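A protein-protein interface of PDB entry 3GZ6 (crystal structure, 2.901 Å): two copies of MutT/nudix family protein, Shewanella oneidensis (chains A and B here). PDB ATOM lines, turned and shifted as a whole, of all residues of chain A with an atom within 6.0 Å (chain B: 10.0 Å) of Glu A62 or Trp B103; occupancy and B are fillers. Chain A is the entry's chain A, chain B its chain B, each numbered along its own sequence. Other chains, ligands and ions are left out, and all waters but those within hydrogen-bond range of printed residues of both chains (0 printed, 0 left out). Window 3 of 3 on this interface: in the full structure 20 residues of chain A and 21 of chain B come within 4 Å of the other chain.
The side-chain carboxylate (OD2) of Asp A65 sits at hydrogen-bond distance from the side-chain hydroxyl (OG1) of Thr A71, 2.8 Å away. The backbone NH (N) of Asp A61 sits at hydrogen-bond distance from the side-chain carboxylate (OD2) of Asp A65 (3.1 Å). The side-chain carboxylate (OE2) of Glu A62 lies close to the side-chain amide nitrogen (NE2) of Gln A21 (3.5 Å). O of Ile A60 sits close to OE1 of Gln A21 (3.0 Å). The side-chain amide oxygen of Asn B95 sits at hydrogen-bond distance from the backbone NH of Arg B98 (3.0 Å). The backbone carbonyl oxygen of Asn B95 sits at hydrogen-bond distance from the backbone NH of Ser B104 (3.2 Å).
Of the 21 printed residues of chain B, 7 touch a printed residue of chain A. Hydrophobic or aromatic side chains of chain B that line the printed part of chain A: Leu B22 and Trp B103. Of the 11 printed residues of chain A, 7 touch a printed residue of chain B. Printed residues of chain A that touch a printed residue of chain B: Gln A21, Ile A60, Glu A62, Asp A65, Glu A66, Ser A67 and Leu A68. Hydrophobic or aromatic side chains of chain A that line the printed part of chain B: Ile A60 and Leu A68. Along chain A the printed residues that touch a printed residue of chain B span positions 21 to 68. Among the printed residues, 14 pairs touch across the chains.
Among the printed residues, pairs that only touch across the chains: Glu A66 with Asn B95 (2.9 Å), Ser A67 with Gly B94 (3.2 Å), Ile A60 with Trp B103 (3.5 Å), Glu A62 with Trp B103 (3.5 Å), Leu A68 with Thr B92 (3.7 Å), Leu A68 with Trp B103 (3.7 Å), Ser A67 with Trp B103 (3.7 Å), Glu A66 with Trp B103 (3.8 Å), Gln A21 with Leu B22 (3.8 Å) and Ser A67 with Asn B95 (3.9 Å).
O of Asp A65 is in hydrogen-bond range of NE1 of Trp B103. The backbone carbonyl oxygen (O) of Gln A21 lies close to the backbone carbonyl oxygen (O) of Gln B21, at 3.0 Å. The backbone NH of Asn B96 lies within hydrogen-bond range of the backbone carbonyl oxygen of Glu A66 (3.2 Å). The backbone NH (N) of Leu A68 sits at hydrogen-bond distance from the backbone carbonyl oxygen (O) of Gly B94, at 2.8 Å.
Asp A61 touches none of the printed residues of chain B. Printed residues of chain B within 4 Å of Glu A62: Trp B103. No residue of chain B comes within 4 Å of Thr A63. No residue of chain B comes within 4 Å of Cys A64. Printed residues of chain B within 4 Å of Asp A65: Trp B103. Printed residues of chain B within 4 Å of Ser A67: Gly B94, Asn B95 and Trp B103. Of chain B, only Thr B92 (3.7 Å), Gly B94 (2.8 Å) and Trp B103 (3.7 Å) come within 4 Å of Leu A68. Thr A71 touches none of the printed residues of chain B. Printed residues of chain A within 4 Å of Gln B21: Gln A21 (3.0 Å). Of the printed residues of chain A, Leu B22 touches Gln A21 (3.8 Å). Of chain A, only Ile A60, Glu A62, Asp A65, Glu A66, Ser A67 and Leu A68 come within 4 Å of Trp B103. The nearest residue of chain B that does not touch Glu A62 is Asn B96 (5.3 Å). The nearest printed residue of chain B that does not touch Ser A67 is Asn B96 (5.4 Å).
Gln B21 touches its own counterpart, Gln A21.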
ATOM      1  N   GLN A  21      -2.937   6.556   5.923  1.00  0.00           N
ATOM      2  CA  GLN A  21      -3.131   5.112   5.851  1.00  0.00           C
ATOM      3  C   GLN A  21      -4.535   4.755   6.350  1.00  0.00           C
ATOM      4  O   GLN A  21      -5.542   5.154   5.714  1.00  0.00           O
ATOM      5  CB  GLN A  21      -2.081   4.364   6.691  1.00  0.00           C
ATOM      6  CG  GLN A  21      -0.667   4.972   6.712  1.00  0.00           C
ATOM      7  CD  GLN A  21       0.075   4.670   8.029  1.00  0.00           C
ATOM      8  OE1 GLN A  21       0.016   3.553   8.547  1.00  0.00           O
ATOM      9  NE2 GLN A  21       0.764   5.671   8.572  1.00  0.00           N
ATOM     10  N   ILE A  60       0.297  -0.631   7.608  1.00  0.00           N
ATOM     11  CA  ILE A  60       1.539  -0.299   6.956  1.00  0.00           C
ATOM     12  C   ILE A  60       2.411   0.458   7.933  1.00  0.00           C
ATOM     13  O   ILE A  60       1.911   1.209   8.760  1.00  0.00           O
ATOM     14  CB  ILE A  60       1.272   0.605   5.776  1.00  0.00           C
ATOM     15  CG1 ILE A  60       0.434  -0.142   4.743  1.00  0.00           C
ATOM     16  CG2 ILE A  60       2.568   1.088   5.186  1.00  0.00           C
ATOM     17  CD1 ILE A  60       0.133   0.690   3.530  1.00  0.00           C
ATOM     18  N   ASP A  61       3.715   0.246   7.840  1.00  0.00           N
ATOM     19  CA  ASP A  61       4.669   0.969   8.657  1.00  0.00           C
ATOM     20  C   ASP A  61       5.620   1.698   7.726  1.00  0.00           C
ATOM     21  O   ASP A  61       6.521   1.094   7.153  1.00  0.00           O
ATOM     22  CB  ASP A  61       5.426   0.007   9.564  1.00  0.00           C
ATOM     23  CG  ASP A  61       6.523   0.691  10.359  1.00  0.00           C
ATOM     24  OD1 ASP A  61       7.081   1.692   9.860  1.00  0.00           O
ATOM     25  OD2 ASP A  61       6.832   0.226  11.482  1.00  0.00           O
ATOM     26  N   GLU A  62       5.422   3.002   7.578  1.00  0.00           N
ATOM     27  CA  GLU A  62       6.143   3.735   6.553  1.00  0.00           C
ATOM     28  C   GLU A  62       7.658   3.845   6.800  1.00  0.00           C
ATOM     29  O   GLU A  62       8.423   4.123   5.879  1.00  0.00           O
ATOM     30  CB  GLU A  62       5.490   5.098   6.335  1.00  0.00           C
ATOM     31  CG  GLU A  62       3.967   5.028   6.349  1.00  0.00           C
ATOM     32  CD  GLU A  62       3.303   6.207   5.653  1.00  0.00           C
ATOM     33  OE1 GLU A  62       4.005   7.197   5.357  1.00  0.00           O
ATOM     34  OE2 GLU A  62       2.074   6.148   5.400  1.00  0.00           O
ATOM     35  N   THR A  63       8.095   3.602   8.029  1.00  0.00           N
ATOM     36  CA  THR A  63       9.523   3.646   8.334  1.00  0.00           C
ATOM     37  C   THR A  63      10.287   2.507   7.653  1.00  0.00           C
ATOM     38  O   THR A  63      11.392   2.705   7.140  1.00  0.00           O
ATOM     39  CB  THR A  63       9.795   3.569   9.856  1.00  0.00           C
ATOM     40  OG1 THR A  63       9.952   2.200  10.250  1.00  0.00           O
ATOM     41  CG2 THR A  63       8.659   4.199  10.652  1.00  0.00           C
ATOM     42  N   CYS A  64       9.693   1.317   7.654  1.00  0.00           N
ATOM     43  CA  CYS A  64      10.357   0.128   7.129  1.00  0.00           C
ATOM     44  C   CYS A  64       9.685  -0.499   5.890  1.00  0.00           C
ATOM     45  O   CYS A  64      10.308  -1.281   5.169  1.00  0.00           O
ATOM     46  CB  CYS A  64      10.500  -0.915   8.234  1.00  0.00           C
ATOM     47  SG  CYS A  64       8.951  -1.314   9.047  1.00  0.00           S
ATOM     48  N   ASP A  65       8.424  -0.163   5.641  1.00  0.00           N
ATOM     49  CA  ASP A  65       7.737  -0.673   4.461  1.00  0.00           C
ATOM     50  C   ASP A  65       7.862   0.317   3.323  1.00  0.00           C
ATOM     51  O   ASP A  65       7.676   1.510   3.511  1.00  0.00           O
ATOM     52  CB  ASP A  65       6.265  -0.953   4.756  1.00  0.00           C
ATOM     53  CG  ASP A  65       6.082  -2.009   5.817  1.00  0.00           C
ATOM     54  OD1 ASP A  65       7.060  -2.728   6.110  1.00  0.00           O
ATOM     55  OD2 ASP A  65       4.964  -2.116   6.357  1.00  0.00           O
ATOM     56  N   GLU A  66       8.184  -0.180   2.139  1.00  0.00           N
ATOM     57  CA  GLU A  66       8.421   0.708   1.012  1.00  0.00           C
ATOM     58  C   GLU A  66       7.471   0.429  -0.141  1.00  0.00           C
ATOM     59  O   GLU A  66       7.200   1.308  -0.947  1.00  0.00           O
ATOM     60  CB  GLU A  66       9.889   0.641   0.590  1.00  0.00           C
ATOM     61  CG  GLU A  66      10.805   1.064   1.739  1.00  0.00           C
ATOM     62  CD  GLU A  66      12.252   1.222   1.336  1.00  0.00           C
ATOM     63  OE1 GLU A  66      12.860   2.243   1.717  1.00  0.00           O
ATOM     64  OE2 GLU A  66      12.783   0.326   0.648  1.00  0.00           O
ATOM     65  N   SER A  67       6.955  -0.792  -0.195  1.00  0.00           N
ATOM     66  CA  SER A  67       5.868  -1.130  -1.096  1.00  0.00           C
ATOM     67  C   SER A  67       4.841  -1.916  -0.293  1.00  0.00           C
ATOM     68  O   SER A  67       5.153  -2.405   0.796  1.00  0.00           O
ATOM     69  CB  SER A  67       6.379  -1.960  -2.270  1.00  0.00           C
ATOM     70  OG  SER A  67       6.673  -3.282  -1.879  1.00  0.00           O
ATOM     71  N   LEU A  68       3.622  -2.027  -0.818  1.00  0.00           N
ATOM     72  CA  LEU A  68       2.571  -2.804  -0.156  1.00  0.00           C
ATOM     73  C   LEU A  68       3.043  -4.225   0.089  1.00  0.00           C
ATOM     74  O   LEU A  68       2.831  -4.784   1.163  1.00  0.00           O
ATOM     75  CB  LEU A  68       1.278  -2.816  -0.989  1.00  0.00           C
ATOM     76  CG  LEU A  68       0.401  -1.560  -0.880  1.00  0.00           C
ATOM     77  CD1 LEU A  68      -0.809  -1.618  -1.786  1.00  0.00           C
ATOM     78  CD2 LEU A  68      -0.045  -1.344   0.552  1.00  0.00           C
ATOM     79  N   THR A  71       5.094  -4.765   3.067  1.00  0.00           N
ATOM     80  CA  THR A  71       4.242  -4.844   4.249  1.00  0.00           C
ATOM     81  C   THR A  71       3.737  -6.260   4.483  1.00  0.00           C
ATOM     82  O   THR A  71       3.969  -6.850   5.535  1.00  0.00           O
ATOM     83  CB  THR A  71       3.015  -3.927   4.131  1.00  0.00           C
ATOM     84  OG1 THR A  71       3.438  -2.563   4.068  1.00  0.00           O
ATOM     85  CG2 THR A  71       2.112  -4.106   5.334  1.00  0.00           C
ATOM     86  N   GLN B  21      -8.781   7.386   5.023  1.00  0.00           N
ATOM     87  CA  GLN B  21      -8.643   7.429   3.572  1.00  0.00           C
ATOM     88  C   GLN B  21      -7.225   7.858   3.196  1.00  0.00           C
ATOM     89  O   GLN B  21      -6.248   7.197   3.606  1.00  0.00           O
ATOM     90  CB  GLN B  21      -9.655   8.396   2.934  1.00  0.00           C
ATOM     91  CG  GLN B  21     -11.059   8.456   3.574  1.00  0.00           C
ATOM     92  CD  GLN B  21     -11.809   9.750   3.205  1.00  0.00           C
ATOM     93  OE1 GLN B  21     -11.456  10.427   2.240  1.00  0.00           O
ATOM     94  NE2 GLN B  21     -12.838  10.095   3.978  1.00  0.00           N
ATOM     95  N   LEU B  22      -7.149   8.977   2.450  1.00  0.00           N
ATOM     96  CA  LEU B  22      -5.923   9.519   1.819  1.00  0.00           C
ATOM     97  C   LEU B  22      -5.602   8.663   0.591  1.00  0.00           C
ATOM     98  O   LEU B  22      -4.652   8.892  -0.162  1.00  0.00           O
ATOM     99  CB  LEU B  22      -4.758   9.600   2.819  1.00  0.00           C
ATOM    100  CG  LEU B  22      -3.282   9.688   2.432  1.00  0.00           C
ATOM    101  CD1 LEU B  22      -2.956  10.930   1.586  1.00  0.00           C
ATOM    102  CD2 LEU B  22      -2.468   9.665   3.721  1.00  0.00           C
ATOM    103  N   LEU B  23      -6.461   7.676   0.396  1.00  0.00           N
ATOM    104  CA  LEU B  23      -6.331   6.694  -0.653  1.00  0.00           C
ATOM    105  C   LEU B  23      -6.989   7.209  -1.928  1.00  0.00           C
ATOM    106  O   LEU B  23      -7.837   8.104  -1.889  1.00  0.00           O
ATOM    107  CB  LEU B  23      -7.032   5.423  -0.178  1.00  0.00           C
ATOM    108  CG  LEU B  23      -7.282   4.297  -1.163  1.00  0.00           C
ATOM    109  CD1 LEU B  23      -5.966   3.650  -1.492  1.00  0.00           C
ATOM    110  CD2 LEU B  23      -8.210   3.303  -0.539  1.00  0.00           C
ATOM    111  N   THR B  24      -6.617   6.626  -3.054  1.00  0.00           N
ATOM    112  CA  THR B  24      -7.196   7.020  -4.320  1.00  0.00           C
ATOM    113  C   THR B  24      -7.780   5.840  -5.091  1.00  0.00           C
ATOM    114  O   THR B  24      -7.320   4.712  -4.950  1.00  0.00           O
ATOM    115  CB  THR B  24      -6.159   7.729  -5.166  1.00  0.00           C
ATOM    116  OG1 THR B  24      -6.370   9.137  -5.050  1.00  0.00           O
ATOM    117  CG2 THR B  24      -6.281   7.313  -6.618  1.00  0.00           C
ATOM    118  N   PHE B  59     -10.518  10.636  -4.698  1.00  0.00           N
ATOM    119  CA  PHE B  59     -10.626  10.202  -3.320  1.00  0.00           C
ATOM    120  C   PHE B  59     -11.940   9.537  -3.090  1.00  0.00           C
ATOM    121  O   PHE B  59     -12.878   9.722  -3.860  1.00  0.00           O
ATOM    122  CB  PHE B  59     -10.486  11.399  -2.387  1.00  0.00           C
ATOM    123  CG  PHE B  59      -9.123  12.009  -2.412  1.00  0.00           C
ATOM    124  CD1 PHE B  59      -8.058  11.367  -1.803  1.00  0.00           C
ATOM    125  CD2 PHE B  59      -8.897  13.204  -3.059  1.00  0.00           C
ATOM    126  CE1 PHE B  59      -6.798  11.917  -1.824  1.00  0.00           C
ATOM    127  CE2 PHE B  59      -7.635  13.759  -3.088  1.00  0.00           C
ATOM    128  CZ  PHE B  59      -6.585  13.118  -2.469  1.00  0.00           C
ATOM    129  N   THR B  92      -3.767  -2.832  -6.967  1.00  0.00           N
ATOM    130  CA  THR B  92      -3.563  -1.698  -6.089  1.00  0.00           C
ATOM    131  C   THR B  92      -2.085  -1.416  -5.974  1.00  0.00           C
ATOM    132  O   THR B  92      -1.304  -2.312  -5.718  1.00  0.00           O
ATOM    133  CB  THR B  92      -4.118  -1.977  -4.699  1.00  0.00           C
ATOM    134  OG1 THR B  92      -5.536  -2.127  -4.788  1.00  0.00           O
ATOM    135  CG2 THR B  92      -3.803  -0.831  -3.764  1.00  0.00           C
ATOM    136  N   VAL B  93      -1.696  -0.169  -6.180  1.00  0.00           N
ATOM    137  CA  VAL B  93      -0.292   0.182  -6.087  1.00  0.00           C
ATOM    138  C   VAL B  93      -0.054   1.025  -4.848  1.00  0.00           C
ATOM    139  O   VAL B  93      -0.812   1.948  -4.551  1.00  0.00           O
ATOM    140  CB  VAL B  93       0.183   0.938  -7.326  1.00  0.00           C
ATOM    141  CG1 VAL B  93       1.677   1.147  -7.259  1.00  0.00           C
ATOM    142  CG2 VAL B  93      -0.165   0.159  -8.565  1.00  0.00           C
ATOM    143  N   GLY B  94       1.006   0.715  -4.119  1.00  0.00           N
ATOM    144  CA  GLY B  94       1.310   1.467  -2.923  1.00  0.00           C
ATOM    145  C   GLY B  94       2.769   1.378  -2.556  1.00  0.00           C
ATOM    146  O   GLY B  94       3.309   0.294  -2.339  1.00  0.00           O
ATOM    147  N   ASN B  95       3.407   2.533  -2.481  1.00  0.00           N
ATOM    148  CA  ASN B  95       4.809   2.595  -2.130  1.00  0.00           C
ATOM    149  C   ASN B  95       5.174   4.039  -1.842  1.00  0.00           C
ATOM    150  O   ASN B  95       4.292   4.886  -1.743  1.00  0.00           O
ATOM    151  CB  ASN B  95       5.629   2.069  -3.286  1.00  0.00           C
ATOM    152  CG  ASN B  95       5.319   2.794  -4.550  1.00  0.00           C
ATOM    153  OD1 ASN B  95       5.346   4.022  -4.577  1.00  0.00           O
ATOM    154  ND2 ASN B  95       4.987   2.057  -5.600  1.00  0.00           N
ATOM    155  N   ASN B  96       6.467   4.323  -1.722  1.00  0.00           N
ATOM    156  CA  ASN B  96       6.917   5.646  -1.296  1.00  0.00           C
ATOM    157  C   ASN B  96       7.664   6.400  -2.379  1.00  0.00           C
ATOM    158  O   ASN B  96       8.361   7.375  -2.111  1.00  0.00           O
ATOM    159  CB  ASN B  96       7.804   5.534  -0.058  1.00  0.00           C
ATOM    160  CG  ASN B  96       8.997   4.627  -0.280  1.00  0.00           C
ATOM    161  OD1 ASN B  96       9.191   4.088  -1.373  1.00  0.00           O
ATOM    162  ND2 ASN B  96       9.800   4.445   0.761  1.00  0.00           N
ATOM    163  N   SER B  97       7.503   5.953  -3.609  1.00  0.00           N
ATOM    164  CA  SER B  97       8.270   6.512  -4.694  1.00  0.00           C
ATOM    165  C   SER B  97       7.385   7.089  -5.797  1.00  0.00           C
ATOM    166  O   SER B  97       7.783   8.018  -6.489  1.00  0.00           O
ATOM    167  CB  SER B  97       9.155   5.428  -5.275  1.00  0.00           C
ATOM    168  OG  SER B  97       8.362   4.395  -5.806  1.00  0.00           O
ATOM    169  N   ARG B  98       6.190   6.536  -5.970  1.00  0.00           N
ATOM    170  CA  ARG B  98       5.331   6.965  -7.064  1.00  0.00           C
ATOM    171  C   ARG B  98       4.922   8.418  -6.882  1.00  0.00           C
ATOM    172  O   ARG B  98       4.659   9.115  -7.862  1.00  0.00           O
ATOM    173  CB  ARG B  98       4.100   6.064  -7.179  1.00  0.00           C
ATOM    174  CG  ARG B  98       3.185   6.112  -5.968  1.00  0.00           C
ATOM    175  CD  ARG B  98       2.186   4.968  -5.998  1.00  0.00           C
ATOM    176  NE  ARG B  98       1.319   5.034  -7.169  1.00  0.00           N
ATOM    177  CZ  ARG B  98       0.110   5.580  -7.161  1.00  0.00           C
ATOM    178  NH1 ARG B  98      -0.371   6.105  -6.044  1.00  0.00           N
ATOM    179  NH2 ARG B  98      -0.621   5.604  -8.262  1.00  0.00           N
ATOM    180  N   ASP B  99       4.878   8.864  -5.628  1.00  0.00           N
ATOM    181  CA  ASP B  99       4.549  10.253  -5.286  1.00  0.00           C
ATOM    182  C   ASP B  99       5.693  10.863  -4.456  1.00  0.00           C
ATOM    183  O   ASP B  99       6.121  10.298  -3.443  1.00  0.00           O
ATOM    184  CB  ASP B  99       3.223  10.302  -4.508  1.00  0.00           C
ATOM    185  CG  ASP B  99       2.654  11.717  -4.367  1.00  0.00           C
ATOM    186  OD1 ASP B  99       1.422  11.870  -4.532  1.00  0.00           O
ATOM    187  OD2 ASP B  99       3.419  12.669  -4.083  1.00  0.00           O
ATOM    188  N   ALA B 100       6.190  12.016  -4.889  1.00  0.00           N
ATOM    189  CA  ALA B 100       7.324  12.647  -4.222  1.00  0.00           C
ATOM    190  C   ALA B 100       6.979  13.121  -2.811  1.00  0.00           C
ATOM    191  O   ALA B 100       7.858  13.300  -1.977  1.00  0.00           O
ATOM    192  CB  ALA B 100       7.842  13.798  -5.053  1.00  0.00           C
ATOM    193  N   ARG B 101       5.696  13.337  -2.554  1.00  0.00           N
ATOM    194  CA  ARG B 101       5.241  13.774  -1.242  1.00  0.00           C
ATOM    195  C   ARG B 101       5.281  12.641  -0.222  1.00  0.00           C
ATOM    196  O   ARG B 101       5.162  12.879   0.976  1.00  0.00           O
ATOM    197  CB  ARG B 101       3.823  14.324  -1.335  1.00  0.00           C
ATOM    198  CG  ARG B 101       3.695  15.506  -2.260  1.00  0.00           C
ATOM    199  CD  ARG B 101       2.234  15.871  -2.466  1.00  0.00           C
ATOM    200  NE  ARG B 101       1.621  15.102  -3.541  1.00  0.00           N
ATOM    201  CZ  ARG B 101       0.310  14.994  -3.722  1.00  0.00           C
ATOM    202  NH1 ARG B 101      -0.526  15.593  -2.888  1.00  0.00           N
ATOM    203  NH2 ARG B 101      -0.169  14.279  -4.728  1.00  0.00           N
ATOM    204  N   GLY B 102       5.438  11.409  -0.696  1.00  0.00           N
ATOM    205  CA  GLY B 102       5.525  10.273   0.201  1.00  0.00           C
ATOM    206  C   GLY B 102       4.603   9.122  -0.146  1.00  0.00           C
ATOM    207  O   GLY B 102       4.234   8.930  -1.308  1.00  0.00           O
ATOM    208  N   TRP B 103       4.236   8.349   0.873  1.00  0.00           N
ATOM    209  CA  TRP B 103       3.452   7.130   0.676  1.00  0.00           C
ATOM    210  C   TRP B 103       2.093   7.431   0.087  1.00  0.00           C
ATOM    211  O   TRP B 103       1.340   8.216   0.638  1.00  0.00           O
ATOM    212  CB  TRP B 103       3.271   6.377   1.993  1.00  0.00           C
ATOM    213  CG  TRP B 103       4.002   5.050   2.080  1.00  0.00           C
ATOM    214  CD1 TRP B 103       5.265   4.840   2.539  1.00  0.00           C
ATOM    215  CD2 TRP B 103       3.490   3.762   1.720  1.00  0.00           C
ATOM    216  NE1 TRP B 103       5.578   3.510   2.474  1.00  0.00           N
ATOM    217  CE2 TRP B 103       4.502   2.824   1.979  1.00  0.00           C
ATOM    218  CE3 TRP B 103       2.276   3.313   1.196  1.00  0.00           C
ATOM    219  CZ2 TRP B 103       4.335   1.461   1.737  1.00  0.00           C
ATOM    220  CZ3 TRP B 103       2.113   1.968   0.962  1.00  0.00           C
ATOM    221  CH2 TRP B 103       3.137   1.055   1.228  1.00  0.00           C
ATOM    222  N   SER B 104       1.787   6.794  -1.035  1.00  0.00           N
ATOM    223  CA  SER B 104       0.507   6.984  -1.688  1.00  0.00           C
ATOM    224  C   SER B 104      -0.054   5.635  -2.107  1.00  0.00           C
ATOM    225  O   SER B 104       0.691   4.724  -2.482  1.00  0.00           O
ATOM    226  CB  SER B 104       0.643   7.903  -2.905  1.00  0.00           C
ATOM    227  OG  SER B 104       1.132   7.210  -4.032  1.00  0.00           O
ATOM    228  N   VAL B 105      -1.370   5.496  -2.037  1.00  0.00           N
ATOM    229  CA  VAL B 105      -1.992   4.268  -2.510  1.00  0.00           C
ATOM    230  C   VAL B 105      -3.122   4.531  -3.492  1.00  0.00           C
ATOM    231  O   VAL B 105      -3.934   5.441  -3.298  1.00  0.00           O
ATOM    232  CB  VAL B 105      -2.549   3.460  -1.366  1.00  0.00           C
ATOM    233  CG1 VAL B 105      -3.057   2.157  -1.898  1.00  0.00           C
ATOM    234  CG2 VAL B 105      -1.484   3.243  -0.316  1.00  0.00           C
ATOM    235  N   THR B 106      -3.156   3.736  -4.553  1.00  0.00           N
ATOM    236  CA  THR B 106      -4.219   3.825  -5.539  1.00  0.00           C
ATOM    237  C   THR B 106      -4.808   2.451  -5.813  1.00  0.00           C
ATOM    238  O   THR B 106      -4.089   1.490  -6.067  1.00  0.00           O
ATOM    239  CB  THR B 106      -3.741   4.452  -6.864  1.00  0.00           C
ATOM    240  OG1 THR B 106      -3.685   5.879  -6.724  1.00  0.00           O
ATOM    241  CG2 THR B 106      -4.699   4.106  -7.978  1.00  0.00           C
ATOM    242  N   PHE B 143       2.264  10.803 -12.337  1.00  0.00           N
ATOM    243  CA  PHE B 143       2.691   9.692 -11.499  1.00  0.00           C
ATOM    244  C   PHE B 143       3.018   8.453 -12.300  1.00  0.00           C
ATOM    245  O   PHE B 143       3.749   8.520 -13.284  1.00  0.00           O
ATOM    246  CB  PHE B 143       1.607   9.383 -10.479  1.00  0.00           C
ATOM    247  CG  PHE B 143       1.170  10.586  -9.702  1.00  0.00           C
ATOM    248  CD1 PHE B 143       2.045  11.216  -8.840  1.00  0.00           C
ATOM    249  CD2 PHE B 143      -0.099  11.105  -9.852  1.00  0.00           C
ATOM    250  CE1 PHE B 143       1.652  12.332  -8.126  1.00  0.00           C
ATOM    251  CE2 PHE B 143      -0.492  12.216  -9.140  1.00  0.00           C
ATOM    252  CZ  PHE B 143       0.387  12.828  -8.276  1.00  0.00           C
